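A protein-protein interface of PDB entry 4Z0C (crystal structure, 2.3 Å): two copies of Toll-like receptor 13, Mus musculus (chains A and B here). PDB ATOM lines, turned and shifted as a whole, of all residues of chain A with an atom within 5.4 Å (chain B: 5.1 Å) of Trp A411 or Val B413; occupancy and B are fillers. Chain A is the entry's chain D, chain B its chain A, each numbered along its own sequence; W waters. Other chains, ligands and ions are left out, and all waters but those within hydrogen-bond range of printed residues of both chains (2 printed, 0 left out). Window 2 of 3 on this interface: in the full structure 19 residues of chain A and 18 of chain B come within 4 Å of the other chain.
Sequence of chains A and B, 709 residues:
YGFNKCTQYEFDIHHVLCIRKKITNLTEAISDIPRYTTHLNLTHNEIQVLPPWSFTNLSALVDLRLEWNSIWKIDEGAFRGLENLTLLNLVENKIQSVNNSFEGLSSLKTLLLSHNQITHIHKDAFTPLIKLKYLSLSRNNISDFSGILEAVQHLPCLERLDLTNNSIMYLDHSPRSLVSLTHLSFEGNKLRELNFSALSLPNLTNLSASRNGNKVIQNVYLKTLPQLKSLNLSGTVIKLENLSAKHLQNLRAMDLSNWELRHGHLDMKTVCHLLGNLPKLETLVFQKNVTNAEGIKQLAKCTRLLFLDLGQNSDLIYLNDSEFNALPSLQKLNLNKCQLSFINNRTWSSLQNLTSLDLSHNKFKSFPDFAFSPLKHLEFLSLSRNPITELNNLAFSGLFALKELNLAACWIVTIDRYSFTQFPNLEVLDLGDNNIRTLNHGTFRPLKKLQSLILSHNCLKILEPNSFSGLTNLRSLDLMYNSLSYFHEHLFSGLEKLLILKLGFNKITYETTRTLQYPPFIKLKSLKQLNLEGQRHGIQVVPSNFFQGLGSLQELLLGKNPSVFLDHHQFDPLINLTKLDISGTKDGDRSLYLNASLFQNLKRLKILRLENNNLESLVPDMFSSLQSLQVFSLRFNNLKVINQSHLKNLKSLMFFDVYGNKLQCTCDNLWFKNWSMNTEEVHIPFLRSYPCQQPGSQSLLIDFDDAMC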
ATOM      1  N   ASN A 386       7.846  22.718   4.804  1.00  0.00           N
ATOM      2  CA  ASN A 386       6.765  23.647   5.074  1.00  0.00           C
ATOM      3  C   ASN A 386       5.570  22.880   5.655  1.00  0.00           C
ATOM      4  O   ASN A 386       5.338  21.730   5.304  1.00  0.00           O
ATOM      5  CB  ASN A 386       6.399  24.428   3.806  1.00  0.00           C
ATOM      6  CG  ASN A 386       7.474  25.436   3.422  1.00  0.00           C
ATOM      7  OD1 ASN A 386       7.613  26.496   4.045  1.00  0.00           O
ATOM      8  ND2 ASN A 386       8.251  25.100   2.400  1.00  0.00           N
ATOM      9  N   PRO A 387       4.840  23.505   6.587  1.00  0.00           N
ATOM     10  CA  PRO A 387       3.647  22.943   7.213  1.00  0.00           C
ATOM     11  C   PRO A 387       2.458  22.957   6.241  1.00  0.00           C
ATOM     12  O   PRO A 387       1.435  23.595   6.480  1.00  0.00           O
ATOM     13  CB  PRO A 387       3.401  23.888   8.388  1.00  0.00           C
ATOM     14  CG  PRO A 387       3.982  25.180   7.970  1.00  0.00           C
ATOM     15  CD  PRO A 387       5.189  24.827   7.143  1.00  0.00           C
ATOM     16  N   ILE A 388       2.647  22.281   5.117  1.00  0.00           N
ATOM     17  CA  ILE A 388       1.657  22.157   4.071  1.00  0.00           C
ATOM     18  C   ILE A 388       0.969  20.818   4.274  1.00  0.00           C
ATOM     19  O   ILE A 388       1.618  19.772   4.214  1.00  0.00           O
ATOM     20  CB  ILE A 388       2.353  22.106   2.699  1.00  0.00           C
ATOM     21  CG1 ILE A 388       3.073  23.422   2.397  1.00  0.00           C
ATOM     22  CG2 ILE A 388       1.369  21.740   1.615  1.00  0.00           C
ATOM     23  CD1 ILE A 388       4.054  23.277   1.305  1.00  0.00           C
ATOM     24  N   THR A 389      -0.339  20.821   4.487  1.00  0.00           N
ATOM     25  CA  THR A 389      -1.046  19.554   4.661  1.00  0.00           C
ATOM     26  C   THR A 389      -1.659  19.083   3.349  1.00  0.00           C
ATOM     27  O   THR A 389      -1.938  17.888   3.169  1.00  0.00           O
ATOM     28  CB  THR A 389      -2.127  19.678   5.707  1.00  0.00           C
ATOM     29  OG1 THR A 389      -2.998  20.759   5.337  1.00  0.00           O
ATOM     30  CG2 THR A 389      -1.511  20.031   7.008  1.00  0.00           C
ATOM     31  N   ALA A 409       9.385  16.120   4.031  1.00  0.00           N
ATOM     32  CA  ALA A 409       9.232  16.659   5.380  1.00  0.00           C
ATOM     33  C   ALA A 409       8.256  17.827   5.507  1.00  0.00           C
ATOM     34  O   ALA A 409       8.350  18.619   6.451  1.00  0.00           O
ATOM     35  CB  ALA A 409      10.603  17.044   5.965  1.00  0.00           C
ATOM     36  N   CYS A 410       7.343  17.949   4.552  1.00  0.00           N
ATOM     37  CA  CYS A 410       6.150  18.774   4.738  1.00  0.00           C
ATOM     38  C   CYS A 410       5.120  17.974   5.564  1.00  0.00           C
ATOM     39  O   CYS A 410       5.453  16.931   6.122  1.00  0.00           O
ATOM     40  CB  CYS A 410       5.575  19.200   3.384  1.00  0.00           C
ATOM     41  SG  CYS A 410       6.625  20.363   2.487  1.00  0.00           S
ATOM     42  N   TRP A 411       3.879  18.440   5.647  1.00  0.00           N
ATOM     43  CA  TRP A 411       2.893  17.736   6.472  1.00  0.00           C
ATOM     44  C   TRP A 411       1.821  17.070   5.625  1.00  0.00           C
ATOM     45  O   TRP A 411       0.697  16.913   6.074  1.00  0.00           O
ATOM     46  CB  TRP A 411       2.224  18.685   7.485  1.00  0.00           C
ATOM     47  CG  TRP A 411       3.178  19.278   8.490  1.00  0.00           C
ATOM     48  CD1 TRP A 411       4.502  18.966   8.649  1.00  0.00           C
ATOM     49  CD2 TRP A 411       2.887  20.294   9.463  1.00  0.00           C
ATOM     50  NE1 TRP A 411       5.042  19.720   9.666  1.00  0.00           N
ATOM     51  CE2 TRP A 411       4.078  20.550  10.172  1.00  0.00           C
ATOM     52  CE3 TRP A 411       1.741  21.018   9.796  1.00  0.00           C
ATOM     53  CZ2 TRP A 411       4.147  21.481  11.209  1.00  0.00           C
ATOM     54  CZ3 TRP A 411       1.814  21.950  10.828  1.00  0.00           C
ATOM     55  CH2 TRP A 411       3.000  22.167  11.522  1.00  0.00           C
ATOM     56  N   ILE A 412       2.164  16.684   4.402  1.00  0.00           N
ATOM     57  CA  ILE A 412       1.138  16.295   3.436  1.00  0.00           C
ATOM     58  C   ILE A 412       0.373  15.039   3.833  1.00  0.00           C
ATOM     59  O   ILE A 412       0.927  13.967   4.067  1.00  0.00           O
ATOM     60  CB  ILE A 412       1.693  16.183   2.015  1.00  0.00           C
ATOM     61  CG1 ILE A 412       2.125  17.558   1.524  1.00  0.00           C
ATOM     62  CG2 ILE A 412       0.676  15.588   1.090  1.00  0.00           C
ATOM     63  CD1 ILE A 412       3.098  17.488   0.369  1.00  0.00           C
ATOM     64  N   VAL A 413      -0.933  15.213   3.848  1.00  0.00           N
ATOM     65  CA  VAL A 413      -1.880  14.317   4.472  1.00  0.00           C
ATOM     66  C   VAL A 413      -2.641  13.530   3.387  1.00  0.00           C
ATOM     67  O   VAL A 413      -3.097  12.420   3.623  1.00  0.00           O
ATOM     68  CB  VAL A 413      -2.796  15.221   5.310  1.00  0.00           C
ATOM     69  CG1 VAL A 413      -4.221  15.317   4.731  1.00  0.00           C
ATOM     70  CG2 VAL A 413      -2.707  14.910   6.758  1.00  0.00           C
ATOM     71  N   ASN A 434       6.392  12.783   4.732  1.00  0.00           N
ATOM     72  CA  ASN A 434       5.102  13.439   4.904  1.00  0.00           C
ATOM     73  C   ASN A 434       4.158  12.642   5.812  1.00  0.00           C
ATOM     74  O   ASN A 434       4.630  11.863   6.635  1.00  0.00           O
ATOM     75  CB  ASN A 434       4.488  13.743   3.553  1.00  0.00           C
ATOM     76  CG  ASN A 434       5.148  14.930   2.899  1.00  0.00           C
ATOM     77  OD1 ASN A 434       4.911  16.084   3.280  1.00  0.00           O
ATOM     78  ND2 ASN A 434       6.021  14.655   1.948  1.00  0.00           N
ATOM     79  N   ASN A 435       2.842  12.818   5.668  1.00  0.00           N
ATOM     80  CA  ASN A 435       1.885  12.087   6.513  1.00  0.00           C
ATOM     81  C   ASN A 435       0.927  11.250   5.680  1.00  0.00           C
ATOM     82  O   ASN A 435      -0.231  11.120   6.018  1.00  0.00           O
ATOM     83  CB  ASN A 435       1.047  13.067   7.340  1.00  0.00           C
ATOM     84  CG  ASN A 435       1.890  13.951   8.238  1.00  0.00           C
ATOM     85  OD1 ASN A 435       2.865  13.499   8.829  1.00  0.00           O
ATOM     86  ND2 ASN A 435       1.522  15.232   8.330  1.00  0.00           N
ATOM     87  N   THR B 389      -7.202  17.649  10.585  1.00  0.00           N
ATOM     88  CA  THR B 389      -5.794  18.010  10.730  1.00  0.00           C
ATOM     89  C   THR B 389      -5.603  19.008  11.862  1.00  0.00           C
ATOM     90  O   THR B 389      -4.504  19.139  12.399  1.00  0.00           O
ATOM     91  CB  THR B 389      -5.205  18.598   9.445  1.00  0.00           C
ATOM     92  OG1 THR B 389      -5.873  19.827   9.126  1.00  0.00           O
ATOM     93  CG2 THR B 389      -5.337  17.609   8.295  1.00  0.00           C
ATOM     94  N   GLU B 390      -6.683  19.685  12.238  1.00  0.00           N
ATOM     95  CA  GLU B 390      -6.604  20.758  13.222  1.00  0.00           C
ATOM     96  C   GLU B 390      -7.885  20.859  14.051  1.00  0.00           C
ATOM     97  O   GLU B 390      -8.982  20.630  13.551  1.00  0.00           O
ATOM     98  CB  GLU B 390      -6.348  22.091  12.502  1.00  0.00           C
ATOM     99  CG  GLU B 390      -4.948  22.645  12.709  1.00  0.00           C
ATOM    100  CD  GLU B 390      -4.663  23.893  11.892  1.00  0.00           C
ATOM    101  OE1 GLU B 390      -4.408  24.951  12.502  1.00  0.00           O
ATOM    102  OE2 GLU B 390      -4.694  23.814  10.644  1.00  0.00           O
ATOM    103  N   TRP B 411      -5.981  12.929  11.806  1.00  0.00           N
ATOM    104  CA  TRP B 411      -4.795  13.360  11.060  1.00  0.00           C
ATOM    105  C   TRP B 411      -4.137  14.569  11.708  1.00  0.00           C
ATOM    106  O   TRP B 411      -3.490  15.375  11.041  1.00  0.00           O
ATOM    107  CB  TRP B 411      -5.155  13.687   9.607  1.00  0.00           C
ATOM    108  CG  TRP B 411      -5.645  12.529   8.807  1.00  0.00           C
ATOM    109  CD1 TRP B 411      -5.711  11.217   9.198  1.00  0.00           C
ATOM    110  CD2 TRP B 411      -6.151  12.575   7.469  1.00  0.00           C
ATOM    111  NE1 TRP B 411      -6.221  10.444   8.178  1.00  0.00           N
ATOM    112  CE2 TRP B 411      -6.506  11.255   7.109  1.00  0.00           C
ATOM    113  CE3 TRP B 411      -6.362  13.604   6.550  1.00  0.00           C
ATOM    114  CZ2 TRP B 411      -7.028  10.939   5.857  1.00  0.00           C
ATOM    115  CZ3 TRP B 411      -6.889  13.289   5.300  1.00  0.00           C
ATOM    116  CH2 TRP B 411      -7.207  11.966   4.964  1.00  0.00           C
ATOM    117  N   ILE B 412      -4.310  14.700  13.011  1.00  0.00           N
ATOM    118  CA  ILE B 412      -3.942  15.937  13.682  1.00  0.00           C
ATOM    119  C   ILE B 412      -2.456  16.283  13.567  1.00  0.00           C
ATOM    120  O   ILE B 412      -1.537  15.490  13.866  1.00  0.00           O
ATOM    121  CB  ILE B 412      -4.416  15.945  15.133  1.00  0.00           C
ATOM    122  CG1 ILE B 412      -5.957  15.964  15.152  1.00  0.00           C
ATOM    123  CG2 ILE B 412      -3.788  17.122  15.897  1.00  0.00           C
ATOM    124  CD1 ILE B 412      -6.566  15.477  16.453  1.00  0.00           C
ATOM    125  N   VAL B 413      -2.253  17.503  13.107  1.00  0.00           N
ATOM    126  CA  VAL B 413      -0.983  17.947  12.603  1.00  0.00           C
ATOM    127  C   VAL B 413      -0.380  18.906  13.620  1.00  0.00           C
ATOM    128  O   VAL B 413       0.827  19.081  13.684  1.00  0.00           O
ATOM    129  CB  VAL B 413      -1.249  18.593  11.228  1.00  0.00           C
ATOM    130  CG1 VAL B 413      -1.024  20.101  11.239  1.00  0.00           C
ATOM    131  CG2 VAL B 413      -0.518  17.854  10.141  1.00  0.00           C
ATOM    132  N   THR B 414      -1.228  19.502  14.453  1.00  0.00           N
ATOM    133  CA  THR B 414      -0.727  20.436  15.450  1.00  0.00           C
ATOM    134  C   THR B 414      -1.763  20.669  16.559  1.00  0.00           C
ATOM    135  O   THR B 414      -2.974  20.615  16.324  1.00  0.00           O
ATOM    136  CB  THR B 414      -0.321  21.781  14.784  1.00  0.00           C
ATOM    137  OG1 THR B 414       0.474  22.570  15.679  1.00  0.00           O
ATOM    138  CG2 THR B 414      -1.546  22.554  14.338  1.00  0.00           C
ATOM    139  N   ILE B 415      -1.276  20.889  17.772  1.00  0.00           N
ATOM    140  CA  ILE B 415      -2.097  21.322  18.896  1.00  0.00           C
ATOM    141  C   ILE B 415      -1.287  22.342  19.694  1.00  0.00           C
ATOM    142  O   ILE B 415      -0.060  22.401  19.574  1.00  0.00           O
ATOM    143  CB  ILE B 415      -2.471  20.132  19.837  1.00  0.00           C
ATOM    144  CG1 ILE B 415      -1.254  19.234  20.098  1.00  0.00           C
ATOM    145  CG2 ILE B 415      -3.575  19.295  19.238  1.00  0.00           C
ATOM    146  CD1 ILE B 415      -1.480  18.175  21.166  1.00  0.00           C
ATOM    147  N   ASN B 435      -0.599  12.820  13.736  1.00  0.00           N
ATOM    148  CA  ASN B 435       0.605  13.225  13.001  1.00  0.00           C
ATOM    149  C   ASN B 435       1.362  14.295  13.769  1.00  0.00           C
ATOM    150  O   ASN B 435       1.914  15.207  13.163  1.00  0.00           O
ATOM    151  CB  ASN B 435       0.250  13.815  11.623  1.00  0.00           C
ATOM    152  CG  ASN B 435      -0.441  12.820  10.703  1.00  0.00           C
ATOM    153  OD1 ASN B 435      -0.080  11.639  10.654  1.00  0.00           O
ATOM    154  ND2 ASN B 435      -1.433  13.297   9.961  1.00  0.00           N
ATOM    155  N   ILE B 436       1.361  14.234  15.093  1.00  0.00           N
ATOM    156  CA  ILE B 436       1.907  15.351  15.848  1.00  0.00           C
ATOM    157  C   ILE B 436       3.410  15.242  15.932  1.00  0.00           C
ATOM    158  O   ILE B 436       3.923  14.203  16.372  1.00  0.00           O
ATOM    159  CB  ILE B 436       1.285  15.456  17.241  1.00  0.00           C
ATOM    160  CG1 ILE B 436      -0.221  15.648  17.110  1.00  0.00           C
ATOM    161  CG2 ILE B 436       1.889  16.623  17.985  1.00  0.00           C
ATOM    162  CD1 ILE B 436      -1.030  15.278  18.362  1.00  0.00           C
ATOM    163  N   ARG B 437       4.109  16.305  15.500  1.00  0.00           N
ATOM    164  CA  ARG B 437       5.582  16.314  15.387  1.00  0.00           C
ATOM    165  C   ARG B 437       6.300  17.017  16.527  1.00  0.00           C
ATOM    166  O   ARG B 437       7.409  16.621  16.896  1.00  0.00           O
ATOM    167  CB  ARG B 437       6.042  16.909  14.048  1.00  0.00           C
ATOM    168  CG  ARG B 437       5.862  15.929  12.915  1.00  0.00           C
ATOM    169  CD  ARG B 437       6.151  16.504  11.540  1.00  0.00           C
ATOM    170  NE  ARG B 437       5.635  15.571  10.545  1.00  0.00           N
ATOM    171  CZ  ARG B 437       6.230  15.277   9.395  1.00  0.00           C
ATOM    172  NH1 ARG B 437       7.369  15.869   9.054  1.00  0.00           N
ATOM    173  NH2 ARG B 437       5.668  14.398   8.576  1.00  0.00           N
HETATM  174  O   HOH W   1      -2.506  11.759   7.884  1.00  0.00           O
HETATM  175  O   HOH W   2       2.727  16.199  10.529  1.00  0.00           O
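The guanidinium group (NH2) of Arg B437 is in hydrogen-bond range of the backbone carbonyl oxygen (O) of Asn A434 (3.4 Å). OD1 of Asn A435 lies within hydrogen-bond range of NH2 of Arg B437, 3.0 Å away.
O of Trp B411 sits at hydrogen-bond distance from ND2 of Asn B435, at 3.1 Å. The backbone carbonyl oxygen (O) of Asn A386 lies close to the side-chain sulfur (SG) of Cys A410, at 3.4 Å. N of Trp A411 lies within hydrogen-bond range of O of Ile A388, at 3.0 Å. The backbone carbonyl oxygen (O) of Thr A389 is in hydrogen-bond range of the backbone NH (N) of Val A413. O of Cys A410 lies close to OD1 of Asn A434 (3.0 Å). N of Asn A435 sits at hydrogen-bond distance from O of Ile A412, 2.7 Å away.
Thr A389 touches Val B413. Arg B437 touches Ala A409 (NH1 to O, 3.9 Å). Cys A410 touches Arg B437. CE3 of Trp A411 touches CG1 of Val B413, at 3.3 Å. NE1 of Trp A411 touches CD of Arg B437, 3.9 Å away. Val A413 touches Trp B411. Val A413 touches Asn B435. Asn A435 touches Val B413 (ND2 to CG2, 3.8 Å). CG of Asn A435 touches CG of Asn B435 (3.6 Å).
Of the printed residues of chain B, Ala A409 touches Arg B437. Of chain B, only Val B413 and Arg B437 come within 4 Å of Trp A411. Of the printed residues of chain B, Asn A434 touches Arg B437 (3.4 Å). Of the printed residues of chain B, Asn A435 touches Val B413, Asn B435 and Arg B437. Val B413 touches just these residues of chain A: Thr A389 (3.9 Å), Trp A411 (3.3 Å) and Asn A435 (3.8 Å). The nearest residue of chain B that does not touch Trp A411 is Thr B414 (4.5 Å). The nearest printed residue of chain B that does not touch Asn A435 is Trp B411 (5.7 Å).
Hydrophobic or aromatic side chains of chain A within 4 Å of the printed part of chain B: Trp A411 and Val A413. Printed residues of chain B that touch a printed residue of chain A: Trp B411, Val B413, Asn B435 and Arg B437. Hydrophobic or aromatic side chains of chain B within 4 Å of the printed part of chain A: Trp B411 and Val B413. Along chain B the printed residues that touch a printed residue of chain A span positions 411 to 437. Among the printed residues, no Asp or Glu carboxylate lies within 4 Å of a Lys or Arg side-chain nitrogen of the other chain.
Thr A389 touches Val B413, but with the chains exchanged Val A413 does not touch Thr B389 (4.1 Å). Trp A411 touches Val B413, and with the chains exchanged Val A413 touches Trp B411. Val A413 touches Asn B435, and with the chains exchanged Asn A435 touches Val B413. Asn A435 touches its own counterpart, Asn B435. Positions printed for both chains: 389, 411, 412, 413 and 435.
Water W2 lies within hydrogen-bond range of ND2 of Asn A435 (2.7 Å), O of Asn B435 (2.9 Å) and NE of Arg B437 (3.0 Å). Water W1 lies within hydrogen-bond range of ND2 of Asn B435 and O of Asn A435.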
